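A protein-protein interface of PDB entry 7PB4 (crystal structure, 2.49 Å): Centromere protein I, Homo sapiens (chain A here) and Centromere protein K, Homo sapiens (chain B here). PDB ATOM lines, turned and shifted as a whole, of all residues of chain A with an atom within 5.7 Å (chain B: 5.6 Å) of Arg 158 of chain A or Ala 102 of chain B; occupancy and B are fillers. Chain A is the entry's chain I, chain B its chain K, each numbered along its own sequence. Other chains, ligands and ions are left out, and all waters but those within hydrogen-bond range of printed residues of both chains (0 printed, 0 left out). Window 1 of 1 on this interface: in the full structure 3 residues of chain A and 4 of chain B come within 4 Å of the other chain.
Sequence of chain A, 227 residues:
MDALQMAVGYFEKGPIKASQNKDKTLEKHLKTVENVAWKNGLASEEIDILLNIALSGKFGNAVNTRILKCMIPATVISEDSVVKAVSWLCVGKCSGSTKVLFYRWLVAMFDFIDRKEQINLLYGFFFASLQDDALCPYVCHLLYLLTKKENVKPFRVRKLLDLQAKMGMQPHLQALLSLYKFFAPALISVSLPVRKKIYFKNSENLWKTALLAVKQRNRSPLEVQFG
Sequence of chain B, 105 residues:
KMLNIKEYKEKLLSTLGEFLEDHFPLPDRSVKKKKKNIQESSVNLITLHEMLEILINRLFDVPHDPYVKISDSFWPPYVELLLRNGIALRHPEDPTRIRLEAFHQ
NH1 of Arg 158 of chain A lies within salt-bridge range of OE1 of Glu 101 of chain B. The guanidinium group (NH2) of Arg 158 of chain A sits at hydrogen-bond distance from the backbone carbonyl oxygen (O) of Ala 102 of chain B, at 3.1 Å. The guanidinium group (NH2) of Arg 158 of chain A is in salt-bridge range of the chain-end carboxylate (OXT) of Gln 105 of chain B. The side-chain amino group of Lys 159 of chain A lies within salt-bridge range of the side-chain carboxylate of Glu 101 of chain B (3.2 Å).
Of chain B, only Glu 101, Ala 102 and Gln 105 come within 4 Å of Arg 158 of chain A. Of chain A, only Arg 158 (3.1 Å) comes within 4 Å of Ala 102 of chain B. Of the printed residues of chain A, Glu 101 of chain B touches Phe 155 (3.9 Å), Arg 158 (3.9 Å) and Lys 159 (3.2 Å). Of the printed residues of chain A, Phe 103 of chain B touches Phe 155. Of the printed residues of chain B, Phe 155 of chain A touches Glu 101 and Phe 103. Printed residues of chain B within 4 Å of Lys 159 of chain A: Glu 101. Leu 59 of chain B touches none of the printed residues of chain A. Leu 100 of chain B touches none of the printed residues of chain A.
Of the 8 printed residues of chain B, 4 touch a printed residue of chain A. Printed residues of chain B that touch a printed residue of chain A: Glu 101, Ala 102, Phe 103 and Gln 105. Hydrophobic or aromatic side chains of chain B that line the printed part of chain A: Phe 103. Of the 11 printed residues of chain A, 3 touch a printed residue of chain B. Hydrophobic or aromatic side chains of chain A within 4 Å of the printed part of chain B: Phe 155. Along chain A the printed residues that touch a printed residue of chain B span positions 155 to 159.
Among the printed residues, pairs that only touch across the chains: Phe 155 of chain A with Phe 103 of chain B and Phe 155 of chain A with Glu 101 of chain B.
The side-chain carboxylate (OD1) of Asp 162 of chain A sits close to the backbone carbonyl oxygen (O) of Arg 158 of chain A, at 2.7 Å.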
ATOM      1  N   LYS A 153      18.077  -1.799  17.581  1.00  0.00           N
ATOM      2  CA  LYS A 153      18.553  -2.976  16.874  1.00  0.00           C
ATOM      3  C   LYS A 153      17.847  -3.117  15.528  1.00  0.00           C
ATOM      4  O   LYS A 153      16.717  -2.644  15.362  1.00  0.00           O
ATOM      5  CB  LYS A 153      18.322  -4.228  17.717  1.00  0.00           C
ATOM      6  CG  LYS A 153      19.081  -4.224  19.037  1.00  0.00           C
ATOM      7  CD  LYS A 153      18.884  -5.522  19.802  1.00  0.00           C
ATOM      8  CE  LYS A 153      19.697  -5.531  21.088  1.00  0.00           C
ATOM      9  NZ  LYS A 153      19.545  -6.812  21.833  1.00  0.00           N
ATOM     10  N   PRO A 154      18.498  -3.751  14.546  1.00  0.00           N
ATOM     11  CA  PRO A 154      17.877  -3.854  13.212  1.00  0.00           C
ATOM     12  C   PRO A 154      16.557  -4.605  13.211  1.00  0.00           C
ATOM     13  O   PRO A 154      15.627  -4.214  12.492  1.00  0.00           O
ATOM     14  CB  PRO A 154      18.946  -4.586  12.389  1.00  0.00           C
ATOM     15  CG  PRO A 154      20.230  -4.318  13.104  1.00  0.00           C
ATOM     16  CD  PRO A 154      19.872  -4.280  14.559  1.00  0.00           C
ATOM     17  N   PHE A 155      16.456  -5.683  13.992  1.00  0.00           N
ATOM     18  CA  PHE A 155      15.202  -6.426  14.073  1.00  0.00           C
ATOM     19  C   PHE A 155      14.069  -5.540  14.569  1.00  0.00           C
ATOM     20  O   PHE A 155      12.949  -5.593  14.043  1.00  0.00           O
ATOM     21  CB  PHE A 155      15.380  -7.641  14.987  1.00  0.00           C
ATOM     22  CG  PHE A 155      14.107  -8.392  15.255  1.00  0.00           C
ATOM     23  CD1 PHE A 155      13.642  -9.333  14.355  1.00  0.00           C
ATOM     24  CD2 PHE A 155      13.382  -8.164  16.414  1.00  0.00           C
ATOM     25  CE1 PHE A 155      12.474 -10.028  14.599  1.00  0.00           C
ATOM     26  CE2 PHE A 155      12.212  -8.855  16.664  1.00  0.00           C
ATOM     27  CZ  PHE A 155      11.758  -9.789  15.756  1.00  0.00           C
ATOM     28  N   ARG A 156      14.342  -4.711  15.578  1.00  0.00           N
ATOM     29  CA  ARG A 156      13.310  -3.832  16.114  1.00  0.00           C
ATOM     30  C   ARG A 156      12.916  -2.760  15.108  1.00  0.00           C
ATOM     31  O   ARG A 156      11.736  -2.408  15.005  1.00  0.00           O
ATOM     32  CB  ARG A 156      13.790  -3.202  17.420  1.00  0.00           C
ATOM     33  CG  ARG A 156      13.878  -4.197  18.556  1.00  0.00           C
ATOM     34  CD  ARG A 156      14.640  -3.637  19.736  1.00  0.00           C
ATOM     35  NE  ARG A 156      14.580  -4.543  20.875  1.00  0.00           N
ATOM     36  CZ  ARG A 156      15.322  -4.418  21.970  1.00  0.00           C
ATOM     37  NH1 ARG A 156      16.192  -3.422  22.073  1.00  0.00           N
ATOM     38  NH2 ARG A 156      15.196  -5.292  22.957  1.00  0.00           N
ATOM     39  N   VAL A 157      13.882  -2.236  14.350  1.00  0.00           N
ATOM     40  CA  VAL A 157      13.559  -1.264  13.309  1.00  0.00           C
ATOM     41  C   VAL A 157      12.666  -1.897  12.250  1.00  0.00           C
ATOM     42  O   VAL A 157      11.672  -1.301  11.814  1.00  0.00           O
ATOM     43  CB  VAL A 157      14.849  -0.690  12.693  1.00  0.00           C
ATOM     44  CG1 VAL A 157      14.515   0.239  11.536  1.00  0.00           C
ATOM     45  CG2 VAL A 157      15.664   0.038  13.751  1.00  0.00           C
ATOM     46  N   ARG A 158      13.001  -3.119  11.827  1.00  0.00           N
ATOM     47  CA  ARG A 158      12.192  -3.810  10.827  1.00  0.00           C
ATOM     48  C   ARG A 158      10.779  -4.062  11.340  1.00  0.00           C
ATOM     49  O   ARG A 158       9.793  -3.815  10.632  1.00  0.00           O
ATOM     50  CB  ARG A 158      12.872  -5.123  10.429  1.00  0.00           C
ATOM     51  CG  ARG A 158      12.054  -6.004   9.499  1.00  0.00           C
ATOM     52  CD  ARG A 158      12.917  -7.089   8.867  1.00  0.00           C
ATOM     53  NE  ARG A 158      13.584  -7.925   9.862  1.00  0.00           N
ATOM     54  CZ  ARG A 158      13.132  -9.107  10.270  1.00  0.00           C
ATOM     55  NH1 ARG A 158      12.007  -9.598   9.769  1.00  0.00           N
ATOM     56  NH2 ARG A 158      13.805  -9.799  11.179  1.00  0.00           N
ATOM     57  N   LYS A 159      10.658  -4.542  12.581  1.00  0.00           N
ATOM     58  CA  LYS A 159       9.337  -4.827  13.133  1.00  0.00           C
ATOM     59  C   LYS A 159       8.525  -3.551  13.326  1.00  0.00           C
ATOM     60  O   LYS A 159       7.308  -3.549  13.115  1.00  0.00           O
ATOM     61  CB  LYS A 159       9.472  -5.591  14.451  1.00  0.00           C
ATOM     62  CG  LYS A 159       9.900  -7.037  14.269  1.00  0.00           C
ATOM     63  CD  LYS A 159       8.966  -7.756  13.305  1.00  0.00           C
ATOM     64  CE  LYS A 159       9.446  -9.166  13.004  1.00  0.00           C
ATOM     65  NZ  LYS A 159       8.558  -9.858  12.030  1.00  0.00           N
ATOM     66  N   LEU A 160       9.180  -2.451  13.706  1.00  0.00           N
ATOM     67  CA  LEU A 160       8.466  -1.189  13.860  1.00  0.00           C
ATOM     68  C   LEU A 160       8.005  -0.651  12.513  1.00  0.00           C
ATOM     69  O   LEU A 160       6.913  -0.081  12.408  1.00  0.00           O
ATOM     70  CB  LEU A 160       9.352  -0.172  14.577  1.00  0.00           C
ATOM     71  CG  LEU A 160       8.638   1.029  15.197  1.00  0.00           C
ATOM     72  CD1 LEU A 160       7.611   0.564  16.220  1.00  0.00           C
ATOM     73  CD2 LEU A 160       9.642   1.976  15.835  1.00  0.00           C
ATOM     74  N   LEU A 161       8.812  -0.837  11.464  1.00  0.00           N
ATOM     75  CA  LEU A 161       8.376  -0.439  10.128  1.00  0.00           C
ATOM     76  C   LEU A 161       7.196  -1.282   9.659  1.00  0.00           C
ATOM     77  O   LEU A 161       6.259  -0.760   9.042  1.00  0.00           O
ATOM     78  CB  LEU A 161       9.540  -0.538   9.142  1.00  0.00           C
ATOM     79  CG  LEU A 161      10.614   0.545   9.263  1.00  0.00           C
ATOM     80  CD1 LEU A 161      11.742   0.300   8.275  1.00  0.00           C
ATOM     81  CD2 LEU A 161      10.007   1.922   9.049  1.00  0.00           C
ATOM     82  N   ASP A 162       7.218  -2.586   9.947  1.00  0.00           N
ATOM     83  CA  ASP A 162       6.080  -3.432   9.592  1.00  0.00           C
ATOM     84  C   ASP A 162       4.828  -3.024  10.362  1.00  0.00           C
ATOM     85  O   ASP A 162       3.721  -3.018   9.809  1.00  0.00           O
ATOM     86  CB  ASP A 162       6.409  -4.905   9.842  1.00  0.00           C
ATOM     87  CG  ASP A 162       7.458  -5.440   8.885  1.00  0.00           C
ATOM     88  OD1 ASP A 162       8.528  -5.880   9.355  1.00  0.00           O
ATOM     89  OD2 ASP A 162       7.216  -5.414   7.660  1.00  0.00           O
ATOM     90  N   LEU A 163       4.983  -2.668  11.639  1.00  0.00           N
ATOM     91  CA  LEU A 163       3.841  -2.214  12.424  1.00  0.00           C
ATOM     92  C   LEU A 163       3.309  -0.883  11.904  1.00  0.00           C
ATOM     93  O   LEU A 163       2.098  -0.641  11.922  1.00  0.00           O
ATOM     94  CB  LEU A 163       4.228  -2.102  13.898  1.00  0.00           C
ATOM     95  CG  LEU A 163       3.095  -1.773  14.870  1.00  0.00           C
ATOM     96  CD1 LEU A 163       1.993  -2.817  14.777  1.00  0.00           C
ATOM     97  CD2 LEU A 163       3.622  -1.675  16.291  1.00  0.00           C
ATOM     98  N   LEU B  59      19.216 -22.320   9.880  1.00  0.00           N
ATOM     99  CA  LEU B  59      19.137 -20.891   9.592  1.00  0.00           C
ATOM    100  C   LEU B  59      20.466 -20.349   9.078  1.00  0.00           C
ATOM    101  O   LEU B  59      20.491 -19.468   8.211  1.00  0.00           O
ATOM    102  CB  LEU B  59      18.693 -20.129  10.840  1.00  0.00           C
ATOM    103  CG  LEU B  59      18.614 -18.606  10.710  1.00  0.00           C
ATOM    104  CD1 LEU B  59      17.675 -18.209   9.581  1.00  0.00           C
ATOM    105  CD2 LEU B  59      18.176 -17.976  12.024  1.00  0.00           C
ATOM    106  N   ARG B  99      10.562 -22.215   9.336  1.00  0.00           N
ATOM    107  CA  ARG B  99      11.882 -21.613   9.437  1.00  0.00           C
ATOM    108  C   ARG B  99      11.983 -20.845  10.745  1.00  0.00           C
ATOM    109  O   ARG B  99      10.989 -20.613  11.436  1.00  0.00           O
ATOM    110  CB  ARG B  99      12.172 -20.678   8.256  1.00  0.00           C
ATOM    111  CG  ARG B  99      11.231 -19.487   8.165  1.00  0.00           C
ATOM    112  CD  ARG B  99      11.845 -18.375   7.334  1.00  0.00           C
ATOM    113  NE  ARG B  99      12.999 -17.783   8.004  1.00  0.00           N
ATOM    114  CZ  ARG B  99      13.831 -16.916   7.437  1.00  0.00           C
ATOM    115  NH1 ARG B  99      13.642 -16.540   6.179  1.00  0.00           N
ATOM    116  NH2 ARG B  99      14.854 -16.429   8.126  1.00  0.00           N
ATOM    117  N   LEU B 100      13.203 -20.442  11.079  1.00  0.00           N
ATOM    118  CA  LEU B 100      13.464 -19.658  12.276  1.00  0.00           C
ATOM    119  C   LEU B 100      13.503 -18.178  11.923  1.00  0.00           C
ATOM    120  O   LEU B 100      14.073 -17.789  10.900  1.00  0.00           O
ATOM    121  CB  LEU B 100      14.783 -20.077  12.927  1.00  0.00           C
ATOM    122  CG  LEU B 100      15.024 -19.544  14.338  1.00  0.00           C
ATOM    123  CD1 LEU B 100      14.044 -20.176  15.311  1.00  0.00           C
ATOM    124  CD2 LEU B 100      16.457 -19.799  14.771  1.00  0.00           C
ATOM    125  N   GLU B 101      12.888 -17.358  12.772  1.00  0.00           N
ATOM    126  CA  GLU B 101      12.902 -15.916  12.562  1.00  0.00           C
ATOM    127  C   GLU B 101      14.325 -15.384  12.670  1.00  0.00           C
ATOM    128  O   GLU B 101      14.999 -15.590  13.684  1.00  0.00           O
ATOM    129  CB  GLU B 101      11.992 -15.229  13.579  1.00  0.00           C
ATOM    130  CG  GLU B 101      12.013 -13.704  13.529  1.00  0.00           C
ATOM    131  CD  GLU B 101      11.328 -13.134  12.298  1.00  0.00           C
ATOM    132  OE1 GLU B 101      11.876 -13.272  11.184  1.00  0.00           O
ATOM    133  OE2 GLU B 101      10.237 -12.545  12.447  1.00  0.00           O
ATOM    134  N   ALA B 102      14.784 -14.707  11.620  1.00  0.00           N
ATOM    135  CA  ALA B 102      16.141 -14.165  11.575  1.00  0.00           C
ATOM    136  C   ALA B 102      16.195 -12.918  12.449  1.00  0.00           C
ATOM    137  O   ALA B 102      15.998 -11.794  11.985  1.00  0.00           O
ATOM    138  CB  ALA B 102      16.554 -13.862  10.139  1.00  0.00           C
ATOM    139  N   PHE B 103      16.466 -13.124  13.738  1.00  0.00           N
ATOM    140  CA  PHE B 103      16.555 -12.014  14.678  1.00  0.00           C
ATOM    141  C   PHE B 103      17.840 -11.211  14.522  1.00  0.00           C
ATOM    142  O   PHE B 103      17.897 -10.066  14.981  1.00  0.00           O
ATOM    143  CB  PHE B 103      16.453 -12.527  16.115  1.00  0.00           C
ATOM    144  CG  PHE B 103      15.150 -13.203  16.428  1.00  0.00           C
ATOM    145  CD1 PHE B 103      13.995 -12.460  16.606  1.00  0.00           C
ATOM    146  CD2 PHE B 103      15.083 -14.579  16.569  1.00  0.00           C
ATOM    147  CE1 PHE B 103      12.795 -13.078  16.905  1.00  0.00           C
ATOM    148  CE2 PHE B 103      13.886 -15.203  16.865  1.00  0.00           C
ATOM    149  CZ  PHE B 103      12.741 -14.451  17.034  1.00  0.00           C
ATOM    150  N   HIS B 104      18.865 -11.783  13.893  1.00  0.00           N
ATOM    151  CA  HIS B 104      20.133 -11.091  13.701  1.00  0.00           C
ATOM    152  C   HIS B 104      20.092 -10.080  12.564  1.00  0.00           C
ATOM    153  O   HIS B 104      21.113  -9.439  12.293  1.00  0.00           O
ATOM    154  CB  HIS B 104      21.251 -12.104  13.445  1.00  0.00           C
ATOM    155  CG  HIS B 104      21.044 -12.931  12.214  1.00  0.00           C
ATOM    156  ND1 HIS B 104      20.257 -14.062  12.202  1.00  0.00           N
ATOM    157  CD2 HIS B 104      21.520 -12.791  10.954  1.00  0.00           C
ATOM    158  CE1 HIS B 104      20.258 -14.585  10.988  1.00  0.00           C
ATOM    159  NE2 HIS B 104      21.017 -13.832  10.213  1.00  0.00           N
ATOM    160  N   GLN B 105      18.952  -9.921  11.899  1.00  0.00           N
ATOM    161  CA  GLN B 105      18.843  -8.999  10.775  1.00  0.00           C
ATOM    162  C   GLN B 105      17.401  -8.535  10.588  1.00  0.00           C
ATOM    163  O   GLN B 105      17.117  -7.661   9.770  1.00  0.00           O
ATOM    164  CB  GLN B 105      19.359  -9.657   9.494  1.00  0.00           C
ATOM    165  CG  GLN B 105      18.620 -10.928   9.104  1.00  0.00           C
ATOM    166  CD  GLN B 105      19.292 -11.669   7.963  1.00  0.00           C
ATOM    167  OE1 GLN B 105      20.433 -11.376   7.603  1.00  0.00           O
ATOM    168  NE2 GLN B 105      18.585 -12.635   7.387  1.00  0.00           N
ATOM    169  OXT GLN B 105      16.486  -9.022  11.253  1.00  0.00           O
